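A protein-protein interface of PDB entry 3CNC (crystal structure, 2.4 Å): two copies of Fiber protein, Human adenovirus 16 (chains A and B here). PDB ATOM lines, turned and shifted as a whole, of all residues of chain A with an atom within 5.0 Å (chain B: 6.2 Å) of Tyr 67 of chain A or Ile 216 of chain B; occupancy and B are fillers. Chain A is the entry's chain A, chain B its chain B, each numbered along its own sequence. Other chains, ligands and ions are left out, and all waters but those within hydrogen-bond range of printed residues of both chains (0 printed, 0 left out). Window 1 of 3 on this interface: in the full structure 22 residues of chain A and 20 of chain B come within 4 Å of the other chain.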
ATOM      1  N   TRP A  31      -4.368  12.195 -32.114  1.00  0.00           N
ATOM      2  CA  TRP A  31      -3.116  12.906 -32.376  1.00  0.00           C
ATOM      3  C   TRP A  31      -2.876  13.355 -33.815  1.00  0.00           C
ATOM      4  O   TRP A  31      -3.688  13.126 -34.709  1.00  0.00           O
ATOM      5  CB  TRP A  31      -1.925  12.039 -31.909  1.00  0.00           C
ATOM      6  CG  TRP A  31      -1.652  10.807 -32.766  1.00  0.00           C
ATOM      7  CD1 TRP A  31      -2.384  10.361 -33.841  1.00  0.00           C
ATOM      8  CD2 TRP A  31      -0.531   9.925 -32.658  1.00  0.00           C
ATOM      9  NE1 TRP A  31      -1.779   9.268 -34.410  1.00  0.00           N
ATOM     10  CE2 TRP A  31      -0.638   8.980 -33.707  1.00  0.00           C
ATOM     11  CE3 TRP A  31       0.561   9.842 -31.781  1.00  0.00           C
ATOM     12  CZ2 TRP A  31       0.316   7.963 -33.905  1.00  0.00           C
ATOM     13  CZ3 TRP A  31       1.509   8.828 -31.977  1.00  0.00           C
ATOM     14  CH2 TRP A  31       1.378   7.905 -33.033  1.00  0.00           C
ATOM     15  N   ALA A  34       2.969  10.700 -35.205  1.00  0.00           N
ATOM     16  CA  ALA A  34       4.301  11.051 -34.727  1.00  0.00           C
ATOM     17  C   ALA A  34       4.968  11.771 -35.912  1.00  0.00           C
ATOM     18  O   ALA A  34       4.568  11.568 -37.070  1.00  0.00           O
ATOM     19  CB  ALA A  34       5.071   9.794 -34.363  1.00  0.00           C
ATOM     20  N   THR A  54       3.103  18.781 -33.304  1.00  0.00           N
ATOM     21  CA  THR A  54       2.907  17.419 -32.814  1.00  0.00           C
ATOM     22  C   THR A  54       2.057  17.536 -31.552  1.00  0.00           C
ATOM     23  O   THR A  54       2.439  18.191 -30.583  1.00  0.00           O
ATOM     24  CB  THR A  54       4.227  16.731 -32.463  1.00  0.00           C
ATOM     25  OG1 THR A  54       5.040  16.650 -33.636  1.00  0.00           O
ATOM     26  CG2 THR A  54       3.969  15.314 -31.957  1.00  0.00           C
ATOM     27  N   LEU A  55       0.889  16.923 -31.572  1.00  0.00           N
ATOM     28  CA  LEU A  55       0.014  16.988 -30.424  1.00  0.00           C
ATOM     29  C   LEU A  55      -0.579  15.615 -30.188  1.00  0.00           C
ATOM     30  O   LEU A  55      -1.130  15.006 -31.100  1.00  0.00           O
ATOM     31  CB  LEU A  55      -1.110  18.003 -30.666  1.00  0.00           C
ATOM     32  CG  LEU A  55      -2.168  18.115 -29.554  1.00  0.00           C
ATOM     33  CD1 LEU A  55      -1.557  18.810 -28.356  1.00  0.00           C
ATOM     34  CD2 LEU A  55      -3.397  18.899 -30.060  1.00  0.00           C
ATOM     35  N   VAL A  56      -0.448  15.123 -28.965  1.00  0.00           N
ATOM     36  CA  VAL A  56      -1.006  13.828 -28.622  1.00  0.00           C
ATOM     37  C   VAL A  56      -1.963  13.974 -27.438  1.00  0.00           C
ATOM     38  O   VAL A  56      -1.580  14.476 -26.375  1.00  0.00           O
ATOM     39  CB  VAL A  56       0.079  12.832 -28.228  1.00  0.00           C
ATOM     40  CG1 VAL A  56      -0.477  11.410 -28.304  1.00  0.00           C
ATOM     41  CG2 VAL A  56       1.297  13.015 -29.127  1.00  0.00           C
ATOM     42  N   ASN A  65      -4.321  12.966 -21.071  1.00  0.00           N
ATOM     43  CA  ASN A  65      -2.892  13.200 -20.882  1.00  0.00           C
ATOM     44  C   ASN A  65      -2.417  13.797 -22.214  1.00  0.00           C
ATOM     45  O   ASN A  65      -2.527  13.145 -23.264  1.00  0.00           O
ATOM     46  CB  ASN A  65      -2.149  11.895 -20.613  1.00  0.00           C
ATOM     47  CG  ASN A  65      -2.203  11.484 -19.163  1.00  0.00           C
ATOM     48  OD1 ASN A  65      -1.725  10.412 -18.810  1.00  0.00           O
ATOM     49  ND2 ASN A  65      -2.779  12.334 -18.308  1.00  0.00           N
ATOM     50  N   GLY A  66      -1.907  15.025 -22.179  1.00  0.00           N
ATOM     51  CA  GLY A  66      -1.469  15.669 -23.409  1.00  0.00           C
ATOM     52  C   GLY A  66       0.025  15.831 -23.610  1.00  0.00           C
ATOM     53  O   GLY A  66       0.783  15.975 -22.651  1.00  0.00           O
ATOM     54  N   TYR A  67       0.434  15.824 -24.879  1.00  0.00           N
ATOM     55  CA  TYR A  67       1.833  15.969 -25.281  1.00  0.00           C
ATOM     56  C   TYR A  67       1.874  16.924 -26.475  1.00  0.00           C
ATOM     57  O   TYR A  67       1.176  16.719 -27.459  1.00  0.00           O
ATOM     58  CB  TYR A  67       2.390  14.606 -25.701  1.00  0.00           C
ATOM     59  CG  TYR A  67       3.799  14.632 -26.262  1.00  0.00           C
ATOM     60  CD1 TYR A  67       4.896  14.355 -25.451  1.00  0.00           C
ATOM     61  CD2 TYR A  67       4.029  14.884 -27.623  1.00  0.00           C
ATOM     62  CE1 TYR A  67       6.193  14.310 -25.975  1.00  0.00           C
ATOM     63  CE2 TYR A  67       5.328  14.850 -28.163  1.00  0.00           C
ATOM     64  CZ  TYR A  67       6.399  14.557 -27.335  1.00  0.00           C
ATOM     65  OH  TYR A  67       7.666  14.470 -27.854  1.00  0.00           O
ATOM     66  N   ILE A  68       2.696  17.964 -26.404  1.00  0.00           N
ATOM     67  CA  ILE A  68       2.751  18.908 -27.510  1.00  0.00           C
ATOM     68  C   ILE A  68       4.135  19.460 -27.760  1.00  0.00           C
ATOM     69  O   ILE A  68       4.875  19.781 -26.825  1.00  0.00           O
ATOM     70  CB  ILE A  68       1.780  20.107 -27.299  1.00  0.00           C
ATOM     71  CG1 ILE A  68       1.719  20.966 -28.566  1.00  0.00           C
ATOM     72  CG2 ILE A  68       2.235  20.953 -26.091  1.00  0.00           C
ATOM     73  CD1 ILE A  68       0.535  21.933 -28.603  1.00  0.00           C
ATOM     74  N   THR A  69       4.450  19.581 -29.045  1.00  0.00           N
ATOM     75  CA  THR A  69       5.727  20.099 -29.489  1.00  0.00           C
ATOM     76  C   THR A  69       5.614  20.791 -30.861  1.00  0.00           C
ATOM     77  O   THR A  69       4.798  20.408 -31.709  1.00  0.00           O
ATOM     78  CB  THR A  69       6.768  18.954 -29.569  1.00  0.00           C
ATOM     79  OG1 THR A  69       8.076  19.501 -29.406  1.00  0.00           O
ATOM     80  CG2 THR A  69       6.681  18.234 -30.901  1.00  0.00           C
ATOM     81  N   GLN A 117       2.435   4.636 -36.121  1.00  0.00           N
ATOM     82  CA  GLN A 117       3.047   5.957 -35.974  1.00  0.00           C
ATOM     83  C   GLN A 117       2.294   7.030 -36.745  1.00  0.00           C
ATOM     84  O   GLN A 117       2.683   8.194 -36.733  1.00  0.00           O
ATOM     85  CB  GLN A 117       4.505   5.928 -36.438  1.00  0.00           C
ATOM     86  CG  GLN A 117       5.393   5.004 -35.629  1.00  0.00           C
ATOM     87  CD  GLN A 117       5.571   5.482 -34.203  1.00  0.00           C
ATOM     88  OE1 GLN A 117       5.163   4.809 -33.244  1.00  0.00           O
ATOM     89  NE2 GLN A 117       6.178   6.649 -34.053  1.00  0.00           N
ATOM     90  N   PRO A 210       9.260  19.090 -25.616  1.00  0.00           N
ATOM     91  CA  PRO A 210       8.010  18.493 -25.140  1.00  0.00           C
ATOM     92  C   PRO A 210       7.355  19.162 -23.937  1.00  0.00           C
ATOM     93  O   PRO A 210       7.974  19.323 -22.888  1.00  0.00           O
ATOM     94  CB  PRO A 210       8.422  17.048 -24.836  1.00  0.00           C
ATOM     95  CG  PRO A 210       9.410  16.769 -25.934  1.00  0.00           C
ATOM     96  CD  PRO A 210      10.253  18.043 -25.926  1.00  0.00           C
ATOM     97  N   PHE A 211       6.099  19.558 -24.098  1.00  0.00           N
ATOM     98  CA  PHE A 211       5.360  20.137 -22.986  1.00  0.00           C
ATOM     99  C   PHE A 211       4.289  19.116 -22.557  1.00  0.00           C
ATOM    100  O   PHE A 211       3.555  18.593 -23.402  1.00  0.00           O
ATOM    101  CB  PHE A 211       4.689  21.451 -23.382  1.00  0.00           C
ATOM    102  CG  PHE A 211       3.861  22.049 -22.278  1.00  0.00           C
ATOM    103  CD1 PHE A 211       4.462  22.482 -21.101  1.00  0.00           C
ATOM    104  CD2 PHE A 211       2.476  22.124 -22.390  1.00  0.00           C
ATOM    105  CE1 PHE A 211       3.695  22.976 -20.053  1.00  0.00           C
ATOM    106  CE2 PHE A 211       1.696  22.619 -21.343  1.00  0.00           C
ATOM    107  CZ  PHE A 211       2.306  23.044 -20.176  1.00  0.00           C
ATOM    108  N   PHE A 212       4.209  18.827 -21.259  1.00  0.00           N
ATOM    109  CA  PHE A 212       3.232  17.852 -20.745  1.00  0.00           C
ATOM    110  C   PHE A 212       2.147  18.548 -19.927  1.00  0.00           C
ATOM    111  O   PHE A 212       2.420  19.529 -19.223  1.00  0.00           O
ATOM    112  CB  PHE A 212       3.925  16.808 -19.857  1.00  0.00           C
ATOM    113  CG  PHE A 212       5.218  16.285 -20.426  1.00  0.00           C
ATOM    114  CD1 PHE A 212       6.409  16.424 -19.714  1.00  0.00           C
ATOM    115  CD2 PHE A 212       5.251  15.672 -21.683  1.00  0.00           C
ATOM    116  CE1 PHE A 212       7.621  15.958 -20.252  1.00  0.00           C
ATOM    117  CE2 PHE A 212       6.451  15.207 -22.226  1.00  0.00           C
ATOM    118  CZ  PHE A 212       7.632  15.348 -21.517  1.00  0.00           C
ATOM    119  N   PHE A 213       0.924  18.030 -20.004  1.00  0.00           N
ATOM    120  CA  PHE A 213      -0.185  18.623 -19.269  1.00  0.00           C
ATOM    121  C   PHE A 213      -1.379  17.680 -19.238  1.00  0.00           C
ATOM    122  O   PHE A 213      -1.433  16.719 -20.003  1.00  0.00           O
ATOM    123  CB  PHE A 213      -0.584  19.947 -19.937  1.00  0.00           C
ATOM    124  CG  PHE A 213      -1.040  19.786 -21.361  1.00  0.00           C
ATOM    125  CD1 PHE A 213      -2.395  19.794 -21.677  1.00  0.00           C
ATOM    126  CD2 PHE A 213      -0.115  19.572 -22.383  1.00  0.00           C
ATOM    127  CE1 PHE A 213      -2.825  19.589 -22.986  1.00  0.00           C
ATOM    128  CE2 PHE A 213      -0.536  19.364 -23.690  1.00  0.00           C
ATOM    129  CZ  PHE A 213      -1.891  19.372 -23.993  1.00  0.00           C
ATOM    130  N   GLY B  62      -0.828   6.215 -27.219  1.00  0.00           N
ATOM    131  CA  GLY B  62       0.363   6.386 -28.036  1.00  0.00           C
ATOM    132  C   GLY B  62       1.549   6.912 -27.238  1.00  0.00           C
ATOM    133  O   GLY B  62       2.644   7.092 -27.773  1.00  0.00           O
ATOM    134  N   LEU B  63       1.341   7.162 -25.951  1.00  0.00           N
ATOM    135  CA  LEU B  63       2.410   7.674 -25.108  1.00  0.00           C
ATOM    136  C   LEU B  63       2.853   6.669 -24.065  1.00  0.00           C
ATOM    137  O   LEU B  63       2.234   5.628 -23.868  1.00  0.00           O
ATOM    138  CB  LEU B  63       1.965   8.936 -24.359  1.00  0.00           C
ATOM    139  CG  LEU B  63       1.514  10.172 -25.141  1.00  0.00           C
ATOM    140  CD1 LEU B  63       0.988  11.230 -24.169  1.00  0.00           C
ATOM    141  CD2 LEU B  63       2.691  10.723 -25.961  1.00  0.00           C
ATOM    142  N   ILE B  64       3.943   7.014 -23.401  1.00  0.00           N
ATOM    143  CA  ILE B  64       4.481   6.239 -22.314  1.00  0.00           C
ATOM    144  C   ILE B  64       4.553   7.273 -21.194  1.00  0.00           C
ATOM    145  O   ILE B  64       5.112   8.356 -21.389  1.00  0.00           O
ATOM    146  CB  ILE B  64       5.912   5.723 -22.622  1.00  0.00           C
ATOM    147  CG1 ILE B  64       5.842   4.528 -23.574  1.00  0.00           C
ATOM    148  CG2 ILE B  64       6.633   5.355 -21.332  1.00  0.00           C
ATOM    149  CD1 ILE B  64       5.129   3.324 -23.006  1.00  0.00           C
ATOM    150  N   MET B 131       9.367   1.252 -25.794  1.00  0.00           N
ATOM    151  CA  MET B 131      10.528   2.016 -26.260  1.00  0.00           C
ATOM    152  C   MET B 131      10.231   3.380 -26.917  1.00  0.00           C
ATOM    153  O   MET B 131       9.138   3.623 -27.443  1.00  0.00           O
ATOM    154  CB  MET B 131      11.344   1.150 -27.232  1.00  0.00           C
ATOM    155  CG  MET B 131      11.951  -0.115 -26.622  1.00  0.00           C
ATOM    156  SD  MET B 131      13.215   0.246 -25.374  1.00  0.00           S
ATOM    157  CE  MET B 131      12.442  -0.401 -23.885  1.00  0.00           C
ATOM    158  N   PRO B 132      11.210   4.297 -26.871  1.00  0.00           N
ATOM    159  CA  PRO B 132      11.059   5.629 -27.470  1.00  0.00           C
ATOM    160  C   PRO B 132      10.893   5.417 -28.973  1.00  0.00           C
ATOM    161  O   PRO B 132      11.662   4.681 -29.573  1.00  0.00           O
ATOM    162  CB  PRO B 132      12.379   6.304 -27.141  1.00  0.00           C
ATOM    163  CG  PRO B 132      12.808   5.634 -25.891  1.00  0.00           C
ATOM    164  CD  PRO B 132      12.480   4.196 -26.138  1.00  0.00           C
ATOM    165  N   SER B 133       9.892   6.041 -29.575  1.00  0.00           N
ATOM    166  CA  SER B 133       9.656   5.882 -31.007  1.00  0.00           C
ATOM    167  C   SER B 133      10.832   6.375 -31.854  1.00  0.00           C
ATOM    168  O   SER B 133      11.318   7.495 -31.643  1.00  0.00           O
ATOM    169  CB  SER B 133       8.396   6.643 -31.417  1.00  0.00           C
ATOM    170  OG  SER B 133       8.202   6.577 -32.813  1.00  0.00           O
ATOM    171  N   ALA B 136       9.558   9.392 -34.043  1.00  0.00           N
ATOM    172  CA  ALA B 136       9.482  10.691 -33.370  1.00  0.00           C
ATOM    173  C   ALA B 136      10.841  11.179 -32.885  1.00  0.00           C
ATOM    174  O   ALA B 136      11.127  12.389 -32.878  1.00  0.00           O
ATOM    175  CB  ALA B 136       8.508  10.615 -32.195  1.00  0.00           C
ATOM    176  N   TYR B 137      11.673  10.241 -32.456  1.00  0.00           N
ATOM    177  CA  TYR B 137      13.006  10.580 -31.983  1.00  0.00           C
ATOM    178  C   TYR B 137      13.973   9.662 -32.744  1.00  0.00           C
ATOM    179  O   TYR B 137      14.267   8.551 -32.312  1.00  0.00           O
ATOM    180  CB  TYR B 137      13.109  10.361 -30.467  1.00  0.00           C
ATOM    181  CG  TYR B 137      11.846  10.722 -29.710  1.00  0.00           C
ATOM    182  CD1 TYR B 137      10.983   9.727 -29.236  1.00  0.00           C
ATOM    183  CD2 TYR B 137      11.485  12.056 -29.511  1.00  0.00           C
ATOM    184  CE1 TYR B 137       9.778  10.058 -28.583  1.00  0.00           C
ATOM    185  CE2 TYR B 137      10.301  12.397 -28.872  1.00  0.00           C
ATOM    186  CZ  TYR B 137       9.443  11.398 -28.411  1.00  0.00           C
ATOM    187  OH  TYR B 137       8.235  11.750 -27.836  1.00  0.00           O
ATOM    188  N   GLU B 149      15.021  17.443 -31.327  1.00  0.00           N
ATOM    189  CA  GLU B 149      13.707  16.941 -30.917  1.00  0.00           C
ATOM    190  C   GLU B 149      13.906  15.718 -30.028  1.00  0.00           C
ATOM    191  O   GLU B 149      12.938  15.184 -29.497  1.00  0.00           O
ATOM    192  CB  GLU B 149      12.867  16.471 -32.103  1.00  0.00           C
ATOM    193  CG  GLU B 149      13.185  17.131 -33.390  1.00  0.00           C
ATOM    194  CD  GLU B 149      14.275  16.422 -34.173  1.00  0.00           C
ATOM    195  OE1 GLU B 149      13.955  15.513 -34.965  1.00  0.00           O
ATOM    196  OE2 GLU B 149      15.447  16.790 -33.986  1.00  0.00           O
ATOM    197  N   ILE B 152      14.245  16.172 -23.797  1.00  0.00           N
ATOM    198  CA  ILE B 152      13.145  16.548 -22.933  1.00  0.00           C
ATOM    199  C   ILE B 152      13.856  17.254 -21.787  1.00  0.00           C
ATOM    200  O   ILE B 152      14.856  16.746 -21.286  1.00  0.00           O
ATOM    201  CB  ILE B 152      12.405  15.297 -22.404  1.00  0.00           C
ATOM    202  CG1 ILE B 152      11.513  14.716 -23.499  1.00  0.00           C
ATOM    203  CG2 ILE B 152      11.590  15.637 -21.157  1.00  0.00           C
ATOM    204  CD1 ILE B 152      10.864  13.392 -23.112  1.00  0.00           C
ATOM    205  N   LEU B 174      16.392  10.868 -25.916  1.00  0.00           N
ATOM    206  CA  LEU B 174      15.716   9.698 -26.452  1.00  0.00           C
ATOM    207  C   LEU B 174      16.410   9.265 -27.738  1.00  0.00           C
ATOM    208  O   LEU B 174      16.544  10.059 -28.676  1.00  0.00           O
ATOM    209  CB  LEU B 174      14.246  10.019 -26.717  1.00  0.00           C
ATOM    210  CG  LEU B 174      13.453  10.469 -25.482  1.00  0.00           C
ATOM    211  CD1 LEU B 174      12.022  10.804 -25.892  1.00  0.00           C
ATOM    212  CD2 LEU B 174      13.462   9.363 -24.420  1.00  0.00           C
ATOM    213  N   SER B 214       6.730  12.237 -20.453  1.00  0.00           N
ATOM    214  CA  SER B 214       6.028  11.404 -21.426  1.00  0.00           C
ATOM    215  C   SER B 214       6.783  11.492 -22.740  1.00  0.00           C
ATOM    216  O   SER B 214       7.504  12.456 -22.964  1.00  0.00           O
ATOM    217  CB  SER B 214       4.611  11.918 -21.659  1.00  0.00           C
ATOM    218  OG  SER B 214       3.933  12.096 -20.440  1.00  0.00           O
ATOM    219  N   TYR B 215       6.621  10.482 -23.590  1.00  0.00           N
ATOM    220  CA  TYR B 215       7.250  10.458 -24.909  1.00  0.00           C
ATOM    221  C   TYR B 215       6.407   9.574 -25.826  1.00  0.00           C
ATOM    222  O   TYR B 215       5.624   8.739 -25.346  1.00  0.00           O
ATOM    223  CB  TYR B 215       8.710   9.972 -24.842  1.00  0.00           C
ATOM    224  CG  TYR B 215       8.936   8.582 -24.278  1.00  0.00           C
ATOM    225  CD1 TYR B 215       8.660   7.442 -25.030  1.00  0.00           C
ATOM    226  CD2 TYR B 215       9.451   8.409 -22.989  1.00  0.00           C
ATOM    227  CE1 TYR B 215       8.893   6.159 -24.511  1.00  0.00           C
ATOM    228  CE2 TYR B 215       9.684   7.132 -22.464  1.00  0.00           C
ATOM    229  CZ  TYR B 215       9.403   6.017 -23.228  1.00  0.00           C
ATOM    230  OH  TYR B 215       9.619   4.765 -22.703  1.00  0.00           O
ATOM    231  N   ILE B 216       6.523   9.807 -27.132  1.00  0.00           N
ATOM    232  CA  ILE B 216       5.767   9.039 -28.118  1.00  0.00           C
ATOM    233  C   ILE B 216       6.397   7.656 -28.105  1.00  0.00           C
ATOM    234  O   ILE B 216       7.618   7.531 -28.113  1.00  0.00           O
ATOM    235  CB  ILE B 216       5.892   9.633 -29.531  1.00  0.00           C
ATOM    236  CG1 ILE B 216       5.532  11.124 -29.511  1.00  0.00           C
ATOM    237  CG2 ILE B 216       5.001   8.863 -30.492  1.00  0.00           C
ATOM    238  CD1 ILE B 216       4.125  11.404 -29.090  1.00  0.00           C
ATOM    239  N   ARG B 217       5.575   6.617 -28.100  1.00  0.00           N
ATOM    240  CA  ARG B 217       6.136   5.282 -28.018  1.00  0.00           C
ATOM    241  C   ARG B 217       6.215   4.496 -29.308  1.00  0.00           C
ATOM    242  O   ARG B 217       5.421   4.682 -30.242  1.00  0.00           O
ATOM    243  CB  ARG B 217       5.374   4.452 -26.966  1.00  0.00           C
ATOM    244  CG  ARG B 217       4.065   3.870 -27.453  1.00  0.00           C
ATOM    245  CD  ARG B 217       3.238   3.292 -26.308  1.00  0.00           C
ATOM    246  NE  ARG B 217       2.047   2.624 -26.820  1.00  0.00           N
ATOM    247  CZ  ARG B 217       2.050   1.396 -27.322  1.00  0.00           C
ATOM    248  NH1 ARG B 217       3.180   0.705 -27.363  1.00  0.00           N
ATOM    249  NH2 ARG B 217       0.936   0.869 -27.806  1.00  0.00           N
ATOM    250  N   GLU B 218       7.195   3.598 -29.313  1.00  0.00           N
ATOM    251  CA  GLU B 218       7.461   2.682 -30.411  1.00  0.00           C
ATOM    252  C   GLU B 218       6.295   1.675 -30.471  1.00  0.00           C
ATOM    253  O   GLU B 218       5.717   1.321 -29.440  1.00  0.00           O
ATOM    254  CB  GLU B 218       8.790   1.970 -30.120  1.00  0.00           C
ATOM    255  CG  GLU B 218       9.269   0.982 -31.154  1.00  0.00           C
ATOM    256  CD  GLU B 218       9.593   1.630 -32.479  1.00  0.00           C
ATOM    257  OE1 GLU B 218      10.267   2.687 -32.486  1.00  0.00           O
ATOM    258  OE2 GLU B 218       9.174   1.071 -33.513  1.00  0.00           O
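Among the printed residues, merely in contact across the chains: Trp 31 of chain A with Ile 216 of chain B, Ala 34 of chain A with Ile 216 of chain B, Val 56 of chain A with Leu 63 of chain B, Val 56 of chain A with Ile 216 of chain B, Tyr 67 of chain A with Leu 63 of chain B, Tyr 67 of chain A with Ser 214 of chain B, Tyr 67 of chain A with Ile 216 of chain B, Pro 210 of chain A with Ile 152 of chain B, Phe 212 of chain A with Ile 152 of chain B and Phe 212 of chain A with Ser 214 of chain B.
The backbone NH (N) of Ala 34 of chain A is in hydrogen-bond range of the backbone carbonyl oxygen (O) of Gln 117 of chain A (2.9 Å). N of Val 56 of chain A is in hydrogen-bond range of O of Tyr 67 of chain A (2.7 Å). N of Arg 217 of chain B is in hydrogen-bond range of O of Gly 62 of chain B, at 3.0 Å. The side-chain hydroxyl (OG) of Ser 133 of chain B lies within hydrogen-bond range of the backbone NH (N) of Ala 136 of chain B. N of Ser 133 of chain B is in hydrogen-bond range of O of Ile 216 of chain B (3.1 Å). OH of Tyr 137 of chain B lies within hydrogen-bond range of N of Ile 216 of chain B (2.7 Å).
OH of Tyr 67 of chain A sits at hydrogen-bond distance from OH of Tyr 137 of chain B, 2.8 Å away. O of Arg 217 of chain B lies close to OE1 of Gln 117 of chain A (3.0 Å). The side-chain hydroxyl (OG) of Ser 133 of chain B lies close to the side-chain amide nitrogen (NE2) of Gln 117 of chain A.
Of the 15 printed residues of chain A, 7 touch a printed residue of chain B. Hydrophobic or aromatic side chains of chain A within 4 Å of the printed part of chain B: Trp 31, Ala 34, Val 56, Tyr 67, Pro 210 and Phe 212. Hydrophobic or aromatic side chains of chain B that line the printed part of chain A: Leu 63, Tyr 137, Ile 152 and Ile 216. Among the printed residues, 13 pairs touch across the chains.
Tyr 67 of chain A touches four residues of chain B. Printed residues of chain A within 4 Å of Ile 216 of chain B: Trp 31 (3.8 Å), Ala 34 (3.98 Å), Val 56 (3.3 Å) and Tyr 67 (3.8 Å). Printed residues of chain A within 4 Å of Arg 217 of chain B: Gln 117 (3.0 Å). Of the printed residues of chain B, Trp 31 of chain A touches Ile 216 (3.8 Å). Printed residues of chain B within 4 Å of Val 56 of chain A: Leu 63 (3.9 Å) and Ile 216 (3.3 Å). Printed residues of chain B within 4 Å of Gln 117 of chain A: Ser 133 (2.4 Å) and Arg 217 (3.0 Å). Printed residues of chain A within 4 Å of Ile 152 of chain B: Pro 210 and Phe 212. The nearest residue of chain B that does not touch Tyr 67 of chain A is Tyr 215 of chain B (4.1 Å). The nearest printed residue of chain A that does not touch Ile 216 of chain B is Gln 117 of chain A (4.4 Å).
No position is printed for both chains.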
